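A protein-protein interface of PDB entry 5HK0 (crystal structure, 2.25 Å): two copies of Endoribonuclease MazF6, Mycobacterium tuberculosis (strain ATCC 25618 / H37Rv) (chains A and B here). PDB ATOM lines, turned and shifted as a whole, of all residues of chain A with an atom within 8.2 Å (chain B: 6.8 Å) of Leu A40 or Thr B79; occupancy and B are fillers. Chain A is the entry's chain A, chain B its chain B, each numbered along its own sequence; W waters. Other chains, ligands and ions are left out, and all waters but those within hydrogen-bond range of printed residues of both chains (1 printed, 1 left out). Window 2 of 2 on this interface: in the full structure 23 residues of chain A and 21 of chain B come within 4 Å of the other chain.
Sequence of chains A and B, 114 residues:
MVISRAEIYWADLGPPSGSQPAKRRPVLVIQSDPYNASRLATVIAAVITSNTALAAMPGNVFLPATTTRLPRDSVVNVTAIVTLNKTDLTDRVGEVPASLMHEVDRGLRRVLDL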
ATOM      1  N   MET A   1      -9.648 -18.876 -14.745  1.00  0.00           N
ATOM      2  CA  MET A   1     -10.743 -19.626 -15.347  1.00  0.00           C
ATOM      3  C   MET A   1     -11.645 -18.735 -16.193  1.00  0.00           C
ATOM      4  O   MET A   1     -11.173 -17.826 -16.878  1.00  0.00           O
ATOM      5  CB  MET A   1     -11.571 -20.326 -14.267  1.00  0.00           C
ATOM      6  CG  MET A   1     -10.978 -21.637 -13.791  1.00  0.00           C
ATOM      7  SD  MET A   1     -10.831 -22.824 -15.139  1.00  0.00           S
ATOM      8  CE  MET A   1     -12.525 -22.893 -15.714  1.00  0.00           C
ATOM      9  N   ILE A   3     -13.531 -16.118 -15.802  1.00  0.00           N
ATOM     10  CA  ILE A   3     -13.902 -14.898 -15.097  1.00  0.00           C
ATOM     11  C   ILE A   3     -14.629 -13.963 -16.053  1.00  0.00           C
ATOM     12  O   ILE A   3     -14.082 -13.565 -17.079  1.00  0.00           O
ATOM     13  CB  ILE A   3     -12.672 -14.190 -14.507  1.00  0.00           C
ATOM     14  CG1 ILE A   3     -11.881 -15.157 -13.624  1.00  0.00           C
ATOM     15  CG2 ILE A   3     -13.093 -12.958 -13.719  1.00  0.00           C
ATOM     16  CD1 ILE A   3     -10.592 -14.583 -13.096  1.00  0.00           C
ATOM     17  N   GLN A  31     -13.623  -5.701 -16.951  1.00  0.00           N
ATOM     18  CA  GLN A  31     -12.914  -6.052 -18.176  1.00  0.00           C
ATOM     19  C   GLN A  31     -13.819  -6.891 -19.071  1.00  0.00           C
ATOM     20  O   GLN A  31     -14.522  -7.781 -18.591  1.00  0.00           O
ATOM     21  CB  GLN A  31     -11.620  -6.807 -17.861  1.00  0.00           C
ATOM     22  CG  GLN A  31     -10.785  -7.141 -19.089  1.00  0.00           C
ATOM     23  CD  GLN A  31      -9.454  -7.777 -18.738  1.00  0.00           C
ATOM     24  OE1 GLN A  31      -8.406  -7.138 -18.828  1.00  0.00           O
ATOM     25  NE2 GLN A  31      -9.488  -9.044 -18.341  1.00  0.00           N
ATOM     26  N   SER A  32     -13.802  -6.605 -20.369  1.00  0.00           N
ATOM     27  CA  SER A  32     -14.691  -7.283 -21.307  1.00  0.00           C
ATOM     28  C   SER A  32     -14.361  -8.767 -21.423  1.00  0.00           C
ATOM     29  O   SER A  32     -13.209  -9.171 -21.276  1.00  0.00           O
ATOM     30  CB  SER A  32     -14.624  -6.627 -22.687  1.00  0.00           C
ATOM     31  OG  SER A  32     -13.532  -7.126 -23.435  1.00  0.00           O
ATOM     32  N   PRO A  34     -14.144 -10.862 -24.006  1.00  0.00           N
ATOM     33  CA  PRO A  34     -13.093 -11.300 -24.936  1.00  0.00           C
ATOM     34  C   PRO A  34     -11.685 -11.265 -24.338  1.00  0.00           C
ATOM     35  O   PRO A  34     -10.939 -12.233 -24.487  1.00  0.00           O
ATOM     36  CB  PRO A  34     -13.215 -10.301 -26.086  1.00  0.00           C
ATOM     37  CG  PRO A  34     -14.652  -9.947 -26.099  1.00  0.00           C
ATOM     38  CD  PRO A  34     -15.073  -9.915 -24.655  1.00  0.00           C
ATOM     39  N   TYR A  35     -11.329 -10.169 -23.672  1.00  0.00           N
ATOM     40  CA  TYR A  35     -10.033 -10.069 -23.008  1.00  0.00           C
ATOM     41  C   TYR A  35      -9.968 -11.028 -21.824  1.00  0.00           C
ATOM     42  O   TYR A  35      -8.903 -11.542 -21.486  1.00  0.00           O
ATOM     43  CB  TYR A  35      -9.768  -8.636 -22.544  1.00  0.00           C
ATOM     44  CG  TYR A  35      -9.573  -7.647 -23.672  1.00  0.00           C
ATOM     45  CD1 TYR A  35     -10.660  -7.060 -24.300  1.00  0.00           C
ATOM     46  CD2 TYR A  35      -8.300  -7.295 -24.102  1.00  0.00           C
ATOM     47  CE1 TYR A  35     -10.491  -6.154 -25.329  1.00  0.00           C
ATOM     48  CE2 TYR A  35      -8.119  -6.388 -25.131  1.00  0.00           C
ATOM     49  CZ  TYR A  35      -9.220  -5.821 -25.741  1.00  0.00           C
ATOM     50  OH  TYR A  35      -9.051  -4.918 -26.765  1.00  0.00           O
ATOM     51  N   ASN A  36     -11.118 -11.260 -21.199  1.00  0.00           N
ATOM     52  CA  ASN A  36     -11.216 -12.213 -20.101  1.00  0.00           C
ATOM     53  C   ASN A  36     -10.970 -13.642 -20.571  1.00  0.00           C
ATOM     54  O   ASN A  36     -10.448 -14.470 -19.826  1.00  0.00           O
ATOM     55  CB  ASN A  36     -12.589 -12.119 -19.431  1.00  0.00           C
ATOM     56  CG  ASN A  36     -12.799 -10.802 -18.710  1.00  0.00           C
ATOM     57  OD1 ASN A  36     -11.850 -10.191 -18.220  1.00  0.00           O
ATOM     58  ND2 ASN A  36     -14.049 -10.360 -18.640  1.00  0.00           N
ATOM     59  N   ALA A  37     -11.354 -13.925 -21.810  1.00  0.00           N
ATOM     60  CA  ALA A  37     -11.185 -15.258 -22.377  1.00  0.00           C
ATOM     61  C   ALA A  37      -9.786 -15.442 -22.959  1.00  0.00           C
ATOM     62  O   ALA A  37      -9.344 -16.568 -23.187  1.00  0.00           O
ATOM     63  CB  ALA A  37     -12.238 -15.516 -23.444  1.00  0.00           C
ATOM     64  N   SER A  38      -9.092 -14.332 -23.189  1.00  0.00           N
ATOM     65  CA  SER A  38      -7.775 -14.370 -23.818  1.00  0.00           C
ATOM     66  C   SER A  38      -6.704 -14.907 -22.876  1.00  0.00           C
ATOM     67  O   SER A  38      -6.998 -15.346 -21.764  1.00  0.00           O
ATOM     68  CB  SER A  38      -7.376 -12.976 -24.308  1.00  0.00           C
ATOM     69  OG  SER A  38      -7.054 -12.126 -23.222  1.00  0.00           O
ATOM     70  N   ARG A  39      -5.457 -14.859 -23.333  1.00  0.00           N
ATOM     71  CA  ARG A  39      -4.333 -15.365 -22.559  1.00  0.00           C
ATOM     72  C   ARG A  39      -3.751 -14.275 -21.667  1.00  0.00           C
ATOM     73  O   ARG A  39      -2.749 -14.488 -20.983  1.00  0.00           O
ATOM     74  CB  ARG A  39      -3.260 -15.929 -23.491  1.00  0.00           C
ATOM     75  CG  ARG A  39      -3.824 -16.848 -24.563  1.00  0.00           C
ATOM     76  CD  ARG A  39      -2.733 -17.571 -25.328  1.00  0.00           C
ATOM     77  NE  ARG A  39      -3.287 -18.398 -26.395  1.00  0.00           N
ATOM     78  CZ  ARG A  39      -2.587 -19.285 -27.096  1.00  0.00           C
ATOM     79  NH1 ARG A  39      -1.299 -19.468 -26.839  1.00  0.00           N
ATOM     80  NH2 ARG A  39      -3.176 -19.993 -28.049  1.00  0.00           N
ATOM     81  N   LEU A  40      -4.386 -13.107 -21.689  1.00  0.00           N
ATOM     82  CA  LEU A  40      -4.020 -12.000 -20.811  1.00  0.00           C
ATOM     83  C   LEU A  40      -4.150 -12.424 -19.351  1.00  0.00           C
ATOM     84  O   LEU A  40      -5.206 -12.880 -18.925  1.00  0.00           O
ATOM     85  CB  LEU A  40      -4.900 -10.780 -21.092  1.00  0.00           C
ATOM     86  CG  LEU A  40      -4.706  -9.539 -20.216  1.00  0.00           C
ATOM     87  CD1 LEU A  40      -3.399  -8.835 -20.544  1.00  0.00           C
ATOM     88  CD2 LEU A  40      -5.888  -8.592 -20.367  1.00  0.00           C
ATOM     89  N   ALA A  41      -3.073 -12.273 -18.589  1.00  0.00           N
ATOM     90  CA  ALA A  41      -3.032 -12.781 -17.223  1.00  0.00           C
ATOM     91  C   ALA A  41      -3.778 -11.893 -16.232  1.00  0.00           C
ATOM     92  O   ALA A  41      -3.995 -12.284 -15.086  1.00  0.00           O
ATOM     93  CB  ALA A  41      -1.587 -12.955 -16.778  1.00  0.00           C
ATOM     94  N   THR A  42      -4.175 -10.702 -16.671  1.00  0.00           N
ATOM     95  CA  THR A  42      -4.743  -9.718 -15.755  1.00  0.00           C
ATOM     96  C   THR A  42      -6.203  -9.369 -16.045  1.00  0.00           C
ATOM     97  O   THR A  42      -6.663  -9.448 -17.185  1.00  0.00           O
ATOM     98  CB  THR A  42      -3.924  -8.415 -15.768  1.00  0.00           C
ATOM     99  OG1 THR A  42      -3.990  -7.818 -17.068  1.00  0.00           O
ATOM    100  CG2 THR A  42      -2.471  -8.696 -15.417  1.00  0.00           C
ATOM    101  N   VAL A  43      -6.919  -8.979 -14.994  1.00  0.00           N
ATOM    102  CA  VAL A  43      -8.312  -8.557 -15.102  1.00  0.00           C
ATOM    103  C   VAL A  43      -8.514  -7.212 -14.408  1.00  0.00           C
ATOM    104  O   VAL A  43      -8.032  -6.998 -13.295  1.00  0.00           O
ATOM    105  CB  VAL A  43      -9.273  -9.598 -14.487  1.00  0.00           C
ATOM    106  CG1 VAL A  43     -10.713  -9.107 -14.555  1.00  0.00           C
ATOM    107  CG2 VAL A  43      -9.137 -10.932 -15.195  1.00  0.00           C
ATOM    108  N   ILE A  44      -9.222  -6.306 -15.076  1.00  0.00           N
ATOM    109  CA  ILE A  44      -9.505  -4.985 -14.528  1.00  0.00           C
ATOM    110  C   ILE A  44     -10.850  -4.978 -13.804  1.00  0.00           C
ATOM    111  O   ILE A  44     -11.840  -5.497 -14.318  1.00  0.00           O
ATOM    112  CB  ILE A  44      -9.505  -3.917 -15.636  1.00  0.00           C
ATOM    113  CG1 ILE A  44      -8.185  -3.957 -16.407  1.00  0.00           C
ATOM    114  CG2 ILE A  44      -9.743  -2.538 -15.053  1.00  0.00           C
ATOM    115  CD1 ILE A  44      -8.157  -3.056 -17.615  1.00  0.00           C
ATOM    116  N   ALA A  45     -10.880  -4.394 -12.610  1.00  0.00           N
ATOM    117  CA  ALA A  45     -12.097  -4.383 -11.805  1.00  0.00           C
ATOM    118  C   ALA A  45     -12.250  -3.094 -11.003  1.00  0.00           C
ATOM    119  O   ALA A  45     -11.270  -2.406 -10.718  1.00  0.00           O
ATOM    120  CB  ALA A  45     -12.116  -5.584 -10.870  1.00  0.00           C
ATOM    121  N   VAL A  82      -8.811  -1.269 -10.222  1.00  0.00           N
ATOM    122  CA  VAL A  82      -7.647  -2.090  -9.901  1.00  0.00           C
ATOM    123  C   VAL A  82      -7.403  -3.173 -10.952  1.00  0.00           C
ATOM    124  O   VAL A  82      -8.346  -3.777 -11.465  1.00  0.00           O
ATOM    125  CB  VAL A  82      -7.809  -2.750  -8.508  1.00  0.00           C
ATOM    126  CG1 VAL A  82      -6.654  -3.691  -8.206  1.00  0.00           C
ATOM    127  CG2 VAL A  82      -7.919  -1.688  -7.428  1.00  0.00           C
ATOM    128  N   THR A  83      -6.133  -3.402 -11.278  1.00  0.00           N
ATOM    129  CA  THR A  83      -5.741  -4.492 -12.167  1.00  0.00           C
ATOM    130  C   THR A  83      -5.253  -5.694 -11.359  1.00  0.00           C
ATOM    131  O   THR A  83      -4.283  -5.594 -10.608  1.00  0.00           O
ATOM    132  CB  THR A  83      -4.635  -4.058 -13.143  1.00  0.00           C
ATOM    133  OG1 THR A  83      -5.096  -2.955 -13.934  1.00  0.00           O
ATOM    134  CG2 THR A  83      -4.253  -5.208 -14.059  1.00  0.00           C
ATOM    135  N   LEU A  84      -5.929  -6.828 -11.518  1.00  0.00           N
ATOM    136  CA  LEU A  84      -5.591  -8.035 -10.767  1.00  0.00           C
ATOM    137  C   LEU A  84      -5.333  -9.221 -11.687  1.00  0.00           C
ATOM    138  O   LEU A  84      -5.821  -9.258 -12.814  1.00  0.00           O
ATOM    139  CB  LEU A  84      -6.710  -8.382  -9.783  1.00  0.00           C
ATOM    140  CG  LEU A  84      -7.008  -7.381  -8.667  1.00  0.00           C
ATOM    141  CD1 LEU A  84      -8.303  -7.747  -7.962  1.00  0.00           C
ATOM    142  CD2 LEU A  84      -5.857  -7.325  -7.677  1.00  0.00           C
ATOM    143  N   ASN A  85      -4.570 -10.193 -11.197  1.00  0.00           N
ATOM    144  CA  ASN A  85      -4.337 -11.427 -11.939  1.00  0.00           C
ATOM    145  C   ASN A  85      -5.579 -12.311 -11.941  1.00  0.00           C
ATOM    146  O   ASN A  85      -6.399 -12.241 -11.027  1.00  0.00           O
ATOM    147  CB  ASN A  85      -3.151 -12.197 -11.353  1.00  0.00           C
ATOM    148  CG  ASN A  85      -1.869 -11.389 -11.355  1.00  0.00           C
ATOM    149  OD1 ASN A  85      -1.673 -10.517 -12.200  1.00  0.00           O
ATOM    150  ND2 ASN A  85      -0.988 -11.680 -10.406  1.00  0.00           N
ATOM    151  N   LYS A  86      -5.710 -13.145 -12.969  1.00  0.00           N
ATOM    152  CA  LYS A  86      -6.843 -14.058 -13.075  1.00  0.00           C
ATOM    153  C   LYS A  86      -6.846 -15.082 -11.946  1.00  0.00           C
ATOM    154  O   LYS A  86      -7.903 -15.515 -11.488  1.00  0.00           O
ATOM    155  CB  LYS A  86      -6.828 -14.780 -14.422  1.00  0.00           C
ATOM    156  CG  LYS A  86      -7.234 -13.910 -15.594  1.00  0.00           C
ATOM    157  CD  LYS A  86      -7.229 -14.695 -16.892  1.00  0.00           C
ATOM    158  CE  LYS A  86      -7.929 -13.923 -17.992  1.00  0.00           C
ATOM    159  NZ  LYS A  86      -7.776 -14.591 -19.315  1.00  0.00           N
ATOM    160  N   THR A  87      -5.654 -15.463 -11.501  1.00  0.00           N
ATOM    161  CA  THR A  87      -5.511 -16.474 -10.461  1.00  0.00           C
ATOM    162  C   THR A  87      -5.895 -15.935  -9.086  1.00  0.00           C
ATOM    163  O   THR A  87      -6.087 -16.702  -8.142  1.00  0.00           O
ATOM    164  CB  THR A  87      -4.071 -17.010 -10.403  1.00  0.00           C
ATOM    165  OG1 THR A  87      -3.177 -15.947 -10.051  1.00  0.00           O
ATOM    166  CG2 THR A  87      -3.664 -17.585 -11.751  1.00  0.00           C
ATOM    167  N   ALA B  46      -3.213   4.828 -16.989  1.00  0.00           N
ATOM    168  CA  ALA B  46      -2.772   3.642 -17.714  1.00  0.00           C
ATOM    169  C   ALA B  46      -1.251   3.549 -17.685  1.00  0.00           C
ATOM    170  O   ALA B  46      -0.556   4.532 -17.941  1.00  0.00           O
ATOM    171  CB  ALA B  46      -3.281   3.670 -19.147  1.00  0.00           C
ATOM    172  N   LEU B  54       4.227  -4.550 -27.042  1.00  0.00           N
ATOM    173  CA  LEU B  54       2.879  -4.541 -26.484  1.00  0.00           C
ATOM    174  C   LEU B  54       1.903  -3.738 -27.340  1.00  0.00           C
ATOM    175  O   LEU B  54       0.703  -3.740 -27.084  1.00  0.00           O
ATOM    176  CB  LEU B  54       2.895  -3.990 -25.058  1.00  0.00           C
ATOM    177  CG  LEU B  54       3.716  -4.787 -24.043  1.00  0.00           C
ATOM    178  CD1 LEU B  54       3.402  -4.337 -22.625  1.00  0.00           C
ATOM    179  CD2 LEU B  54       3.474  -6.281 -24.200  1.00  0.00           C
ATOM    180  N   MET B  57      -0.868  -5.784 -29.087  1.00  0.00           N
ATOM    181  CA  MET B  57      -2.102  -6.094 -28.375  1.00  0.00           C
ATOM    182  C   MET B  57      -3.203  -5.141 -28.835  1.00  0.00           C
ATOM    183  O   MET B  57      -2.947  -3.953 -29.027  1.00  0.00           O
ATOM    184  CB  MET B  57      -1.894  -5.999 -26.862  1.00  0.00           C
ATOM    185  CG  MET B  57      -0.587  -6.609 -26.372  1.00  0.00           C
ATOM    186  SD  MET B  57      -0.218  -8.217 -27.104  1.00  0.00           S
ATOM    187  CE  MET B  57      -1.563  -9.212 -26.461  1.00  0.00           C
ATOM    188  N   GLY B  59      -6.046  -3.346 -27.845  1.00  0.00           N
ATOM    189  CA  GLY B  59      -6.396  -2.037 -27.321  1.00  0.00           C
ATOM    190  C   GLY B  59      -5.238  -1.065 -27.191  1.00  0.00           C
ATOM    191  O   GLY B  59      -5.444   0.148 -27.149  1.00  0.00           O
ATOM    192  N   ASN B  60      -4.021  -1.596 -27.124  1.00  0.00           N
ATOM    193  CA  ASN B  60      -2.835  -0.777 -26.895  1.00  0.00           C
ATOM    194  C   ASN B  60      -2.531   0.178 -28.043  1.00  0.00           C
ATOM    195  O   ASN B  60      -2.699  -0.168 -29.212  1.00  0.00           O
ATOM    196  CB  ASN B  60      -1.624  -1.671 -26.643  1.00  0.00           C
ATOM    197  CG  ASN B  60      -1.814  -2.588 -25.454  1.00  0.00           C
ATOM    198  OD1 ASN B  60      -2.901  -2.667 -24.882  1.00  0.00           O
ATOM    199  ND2 ASN B  60      -0.755  -3.295 -25.076  1.00  0.00           N
ATOM    200  N   VAL B  76       1.094   2.621 -24.710  1.00  0.00           N
ATOM    201  CA  VAL B  76       0.079   2.659 -23.664  1.00  0.00           C
ATOM    202  C   VAL B  76      -0.565   1.290 -23.492  1.00  0.00           C
ATOM    203  O   VAL B  76      -1.175   0.760 -24.420  1.00  0.00           O
ATOM    204  CB  VAL B  76      -1.019   3.696 -23.971  1.00  0.00           C
ATOM    205  CG1 VAL B  76      -2.171   3.557 -22.988  1.00  0.00           C
ATOM    206  CG2 VAL B  76      -0.446   5.100 -23.933  1.00  0.00           C
ATOM    207  N   ASN B  77      -0.421   0.715 -22.302  1.00  0.00           N
ATOM    208  CA  ASN B  77      -1.036  -0.572 -22.006  1.00  0.00           C
ATOM    209  C   ASN B  77      -2.394  -0.380 -21.341  1.00  0.00           C
ATOM    210  O   ASN B  77      -2.484  -0.176 -20.131  1.00  0.00           O
ATOM    211  CB  ASN B  77      -0.119  -1.416 -21.116  1.00  0.00           C
ATOM    212  CG  ASN B  77      -0.578  -2.859 -21.007  1.00  0.00           C
ATOM    213  OD1 ASN B  77      -1.480  -3.293 -21.724  1.00  0.00           O
ATOM    214  ND2 ASN B  77       0.049  -3.613 -20.112  1.00  0.00           N
ATOM    215  N   VAL B  78      -3.449  -0.447 -22.147  1.00  0.00           N
ATOM    216  CA  VAL B  78      -4.806  -0.203 -21.671  1.00  0.00           C
ATOM    217  C   VAL B  78      -5.356  -1.374 -20.860  1.00  0.00           C
ATOM    218  O   VAL B  78      -6.451  -1.292 -20.302  1.00  0.00           O
ATOM    219  CB  VAL B  78      -5.761   0.083 -22.841  1.00  0.00           C
ATOM    220  CG1 VAL B  78      -5.377   1.383 -23.532  1.00  0.00           C
ATOM    221  CG2 VAL B  78      -5.740  -1.073 -23.823  1.00  0.00           C
ATOM    222  N   THR B  79      -4.596  -2.462 -20.804  1.00  0.00           N
ATOM    223  CA  THR B  79      -4.981  -3.625 -20.014  1.00  0.00           C
ATOM    224  C   THR B  79      -4.452  -3.500 -18.589  1.00  0.00           C
ATOM    225  O   THR B  79      -4.870  -4.235 -17.693  1.00  0.00           O
ATOM    226  CB  THR B  79      -4.463  -4.933 -20.639  1.00  0.00           C
ATOM    227  OG1 THR B  79      -3.030  -4.916 -20.674  1.00  0.00           O
ATOM    228  CG2 THR B  79      -4.999  -5.098 -22.053  1.00  0.00           C
ATOM    229  N   ALA B  80      -3.528  -2.566 -18.389  1.00  0.00           N
ATOM    230  CA  ALA B  80      -2.956  -2.312 -17.071  1.00  0.00           C
ATOM    231  C   ALA B  80      -3.406  -0.956 -16.538  1.00  0.00           C
ATOM    232  O   ALA B  80      -2.779   0.069 -16.806  1.00  0.00           O
ATOM    233  CB  ALA B  80      -1.439  -2.382 -17.126  1.00  0.00           C
ATOM    234  N   ILE B  81      -4.500  -0.958 -15.783  1.00  0.00           N
ATOM    235  CA  ILE B  81      -5.056   0.271 -15.233  1.00  0.00           C
ATOM    236  C   ILE B  81      -4.845   0.351 -13.725  1.00  0.00           C
ATOM    237  O   ILE B  81      -5.239  -0.551 -12.986  1.00  0.00           O
ATOM    238  CB  ILE B  81      -6.560   0.393 -15.537  1.00  0.00           C
ATOM    239  CG1 ILE B  81      -6.801   0.375 -17.047  1.00  0.00           C
ATOM    240  CG2 ILE B  81      -7.126   1.660 -14.924  1.00  0.00           C
ATOM    241  CD1 ILE B  81      -8.245   0.595 -17.434  1.00  0.00           C
ATOM    242  N   LEU B 108      -9.724   1.758 -24.930  1.00  0.00           N
ATOM    243  CA  LEU B 108     -10.222   1.734 -23.561  1.00  0.00           C
ATOM    244  C   LEU B 108     -11.635   1.163 -23.510  1.00  0.00           C
ATOM    245  O   LEU B 108     -12.020   0.516 -22.537  1.00  0.00           O
ATOM    246  CB  LEU B 108     -10.201   3.142 -22.962  1.00  0.00           C
ATOM    247  CG  LEU B 108      -9.685   3.291 -21.532  1.00  0.00           C
ATOM    248  CD1 LEU B 108      -8.285   2.711 -21.408  1.00  0.00           C
ATOM    249  CD2 LEU B 108      -9.697   4.753 -21.121  1.00  0.00           C
ATOM    250  N   VAL B 111     -11.538  -2.846 -24.039  1.00  0.00           N
ATOM    251  CA  VAL B 111     -11.084  -3.576 -22.862  1.00  0.00           C
ATOM    252  C   VAL B 111     -12.127  -3.575 -21.746  1.00  0.00           C
ATOM    253  O   VAL B 111     -12.294  -4.569 -21.039  1.00  0.00           O
ATOM    254  CB  VAL B 111      -9.763  -2.986 -22.327  1.00  0.00           C
ATOM    255  CG1 VAL B 111      -9.317  -3.707 -21.066  1.00  0.00           C
ATOM    256  CG2 VAL B 111      -8.689  -3.071 -23.394  1.00  0.00           C
HETATM  257  O   HOH W   1      -4.140  -1.712 -10.790  1.00  0.00           O
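Printed residues of chain B within 4 Å of Leu A40: Thr B79 (3.9 Å). Thr B79 touches four residues of chain A. Of the printed residues of chain A, Val B111 touches Gln A31, Ser A32, Tyr A35 and Ile A44. Printed residues of chain B within 4 Å of Tyr A35: Gly B59 and Val B111. Ala B46 touches none of the printed residues of chain A. The nearest printed residue of chain B that does not touch Leu A40 is Asn B77 (6.0 Å). The nearest residue of chain A that does not touch Thr B79 is Tyr A35 (4.5 Å). The nearest printed residue of chain A that does not touch Ile B81 is Leu A84 (6.5 Å).
Water W1 bridges N of Thr A83 (2.7 Å) and O of Ile B81 (2.7 Å).
O of Val B111 lies within hydrogen-bond range of N of Ser A32, 2.6 Å away. OG1 of Thr A83 lies within hydrogen-bond range of O of Ile B81, at 2.6 Å.
O of Gln A31 is in hydrogen-bond range of ND2 of Asn A36 (2.6 Å). The side-chain amide nitrogen (NE2) of Gln A31 is in hydrogen-bond range of the backbone carbonyl oxygen (O) of Thr A42 (3.1 Å). The backbone NH (N) of Gln A31 sits at hydrogen-bond distance from the backbone carbonyl oxygen (O) of Ile A44 (3.2 Å). ND2 of Asn A36 lies within hydrogen-bond range of O of Ser A32 (3.0 Å). The backbone carbonyl oxygen (O) of Leu A40 lies close to the side-chain amino group (NZ) of Lys A86 (3.1 Å). The backbone carbonyl oxygen of Ala A45 lies within hydrogen-bond range of the backbone NH of Val A82, 2.8 Å away.
Of the 13 printed residues of chain B, 6 touch a printed residue of chain A. Hydrophobic or aromatic side chains of chain B within 4 Å of the printed part of chain A: Ile B81 and Val B111. Among the printed residues, 14 pairs touch across the chains. Among the printed residues, no Asp or Glu carboxylate lies within 4 Å of a Lys or Arg side-chain nitrogen of the other chain.
Among the printed residues, pairs that only touch across the chains: Gln A31 with Val B111, Ile A44 with Thr B79, Tyr A35 with Gly B59, Tyr A35 with Val B111, Ile A44 with Val B78, Ile A44 with Ile B81, Thr A83 with Ala B80, Ile A44 with Val B111, Thr A42 with Thr B79, Thr A83 with Thr B79, Leu A40 with Thr B79 and Val A82 with Ile B81.
No position is printed for both chains. Of the 14 pairs that touch across the chains among the printed residues, none has its exchanged pair printed and touching as well.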
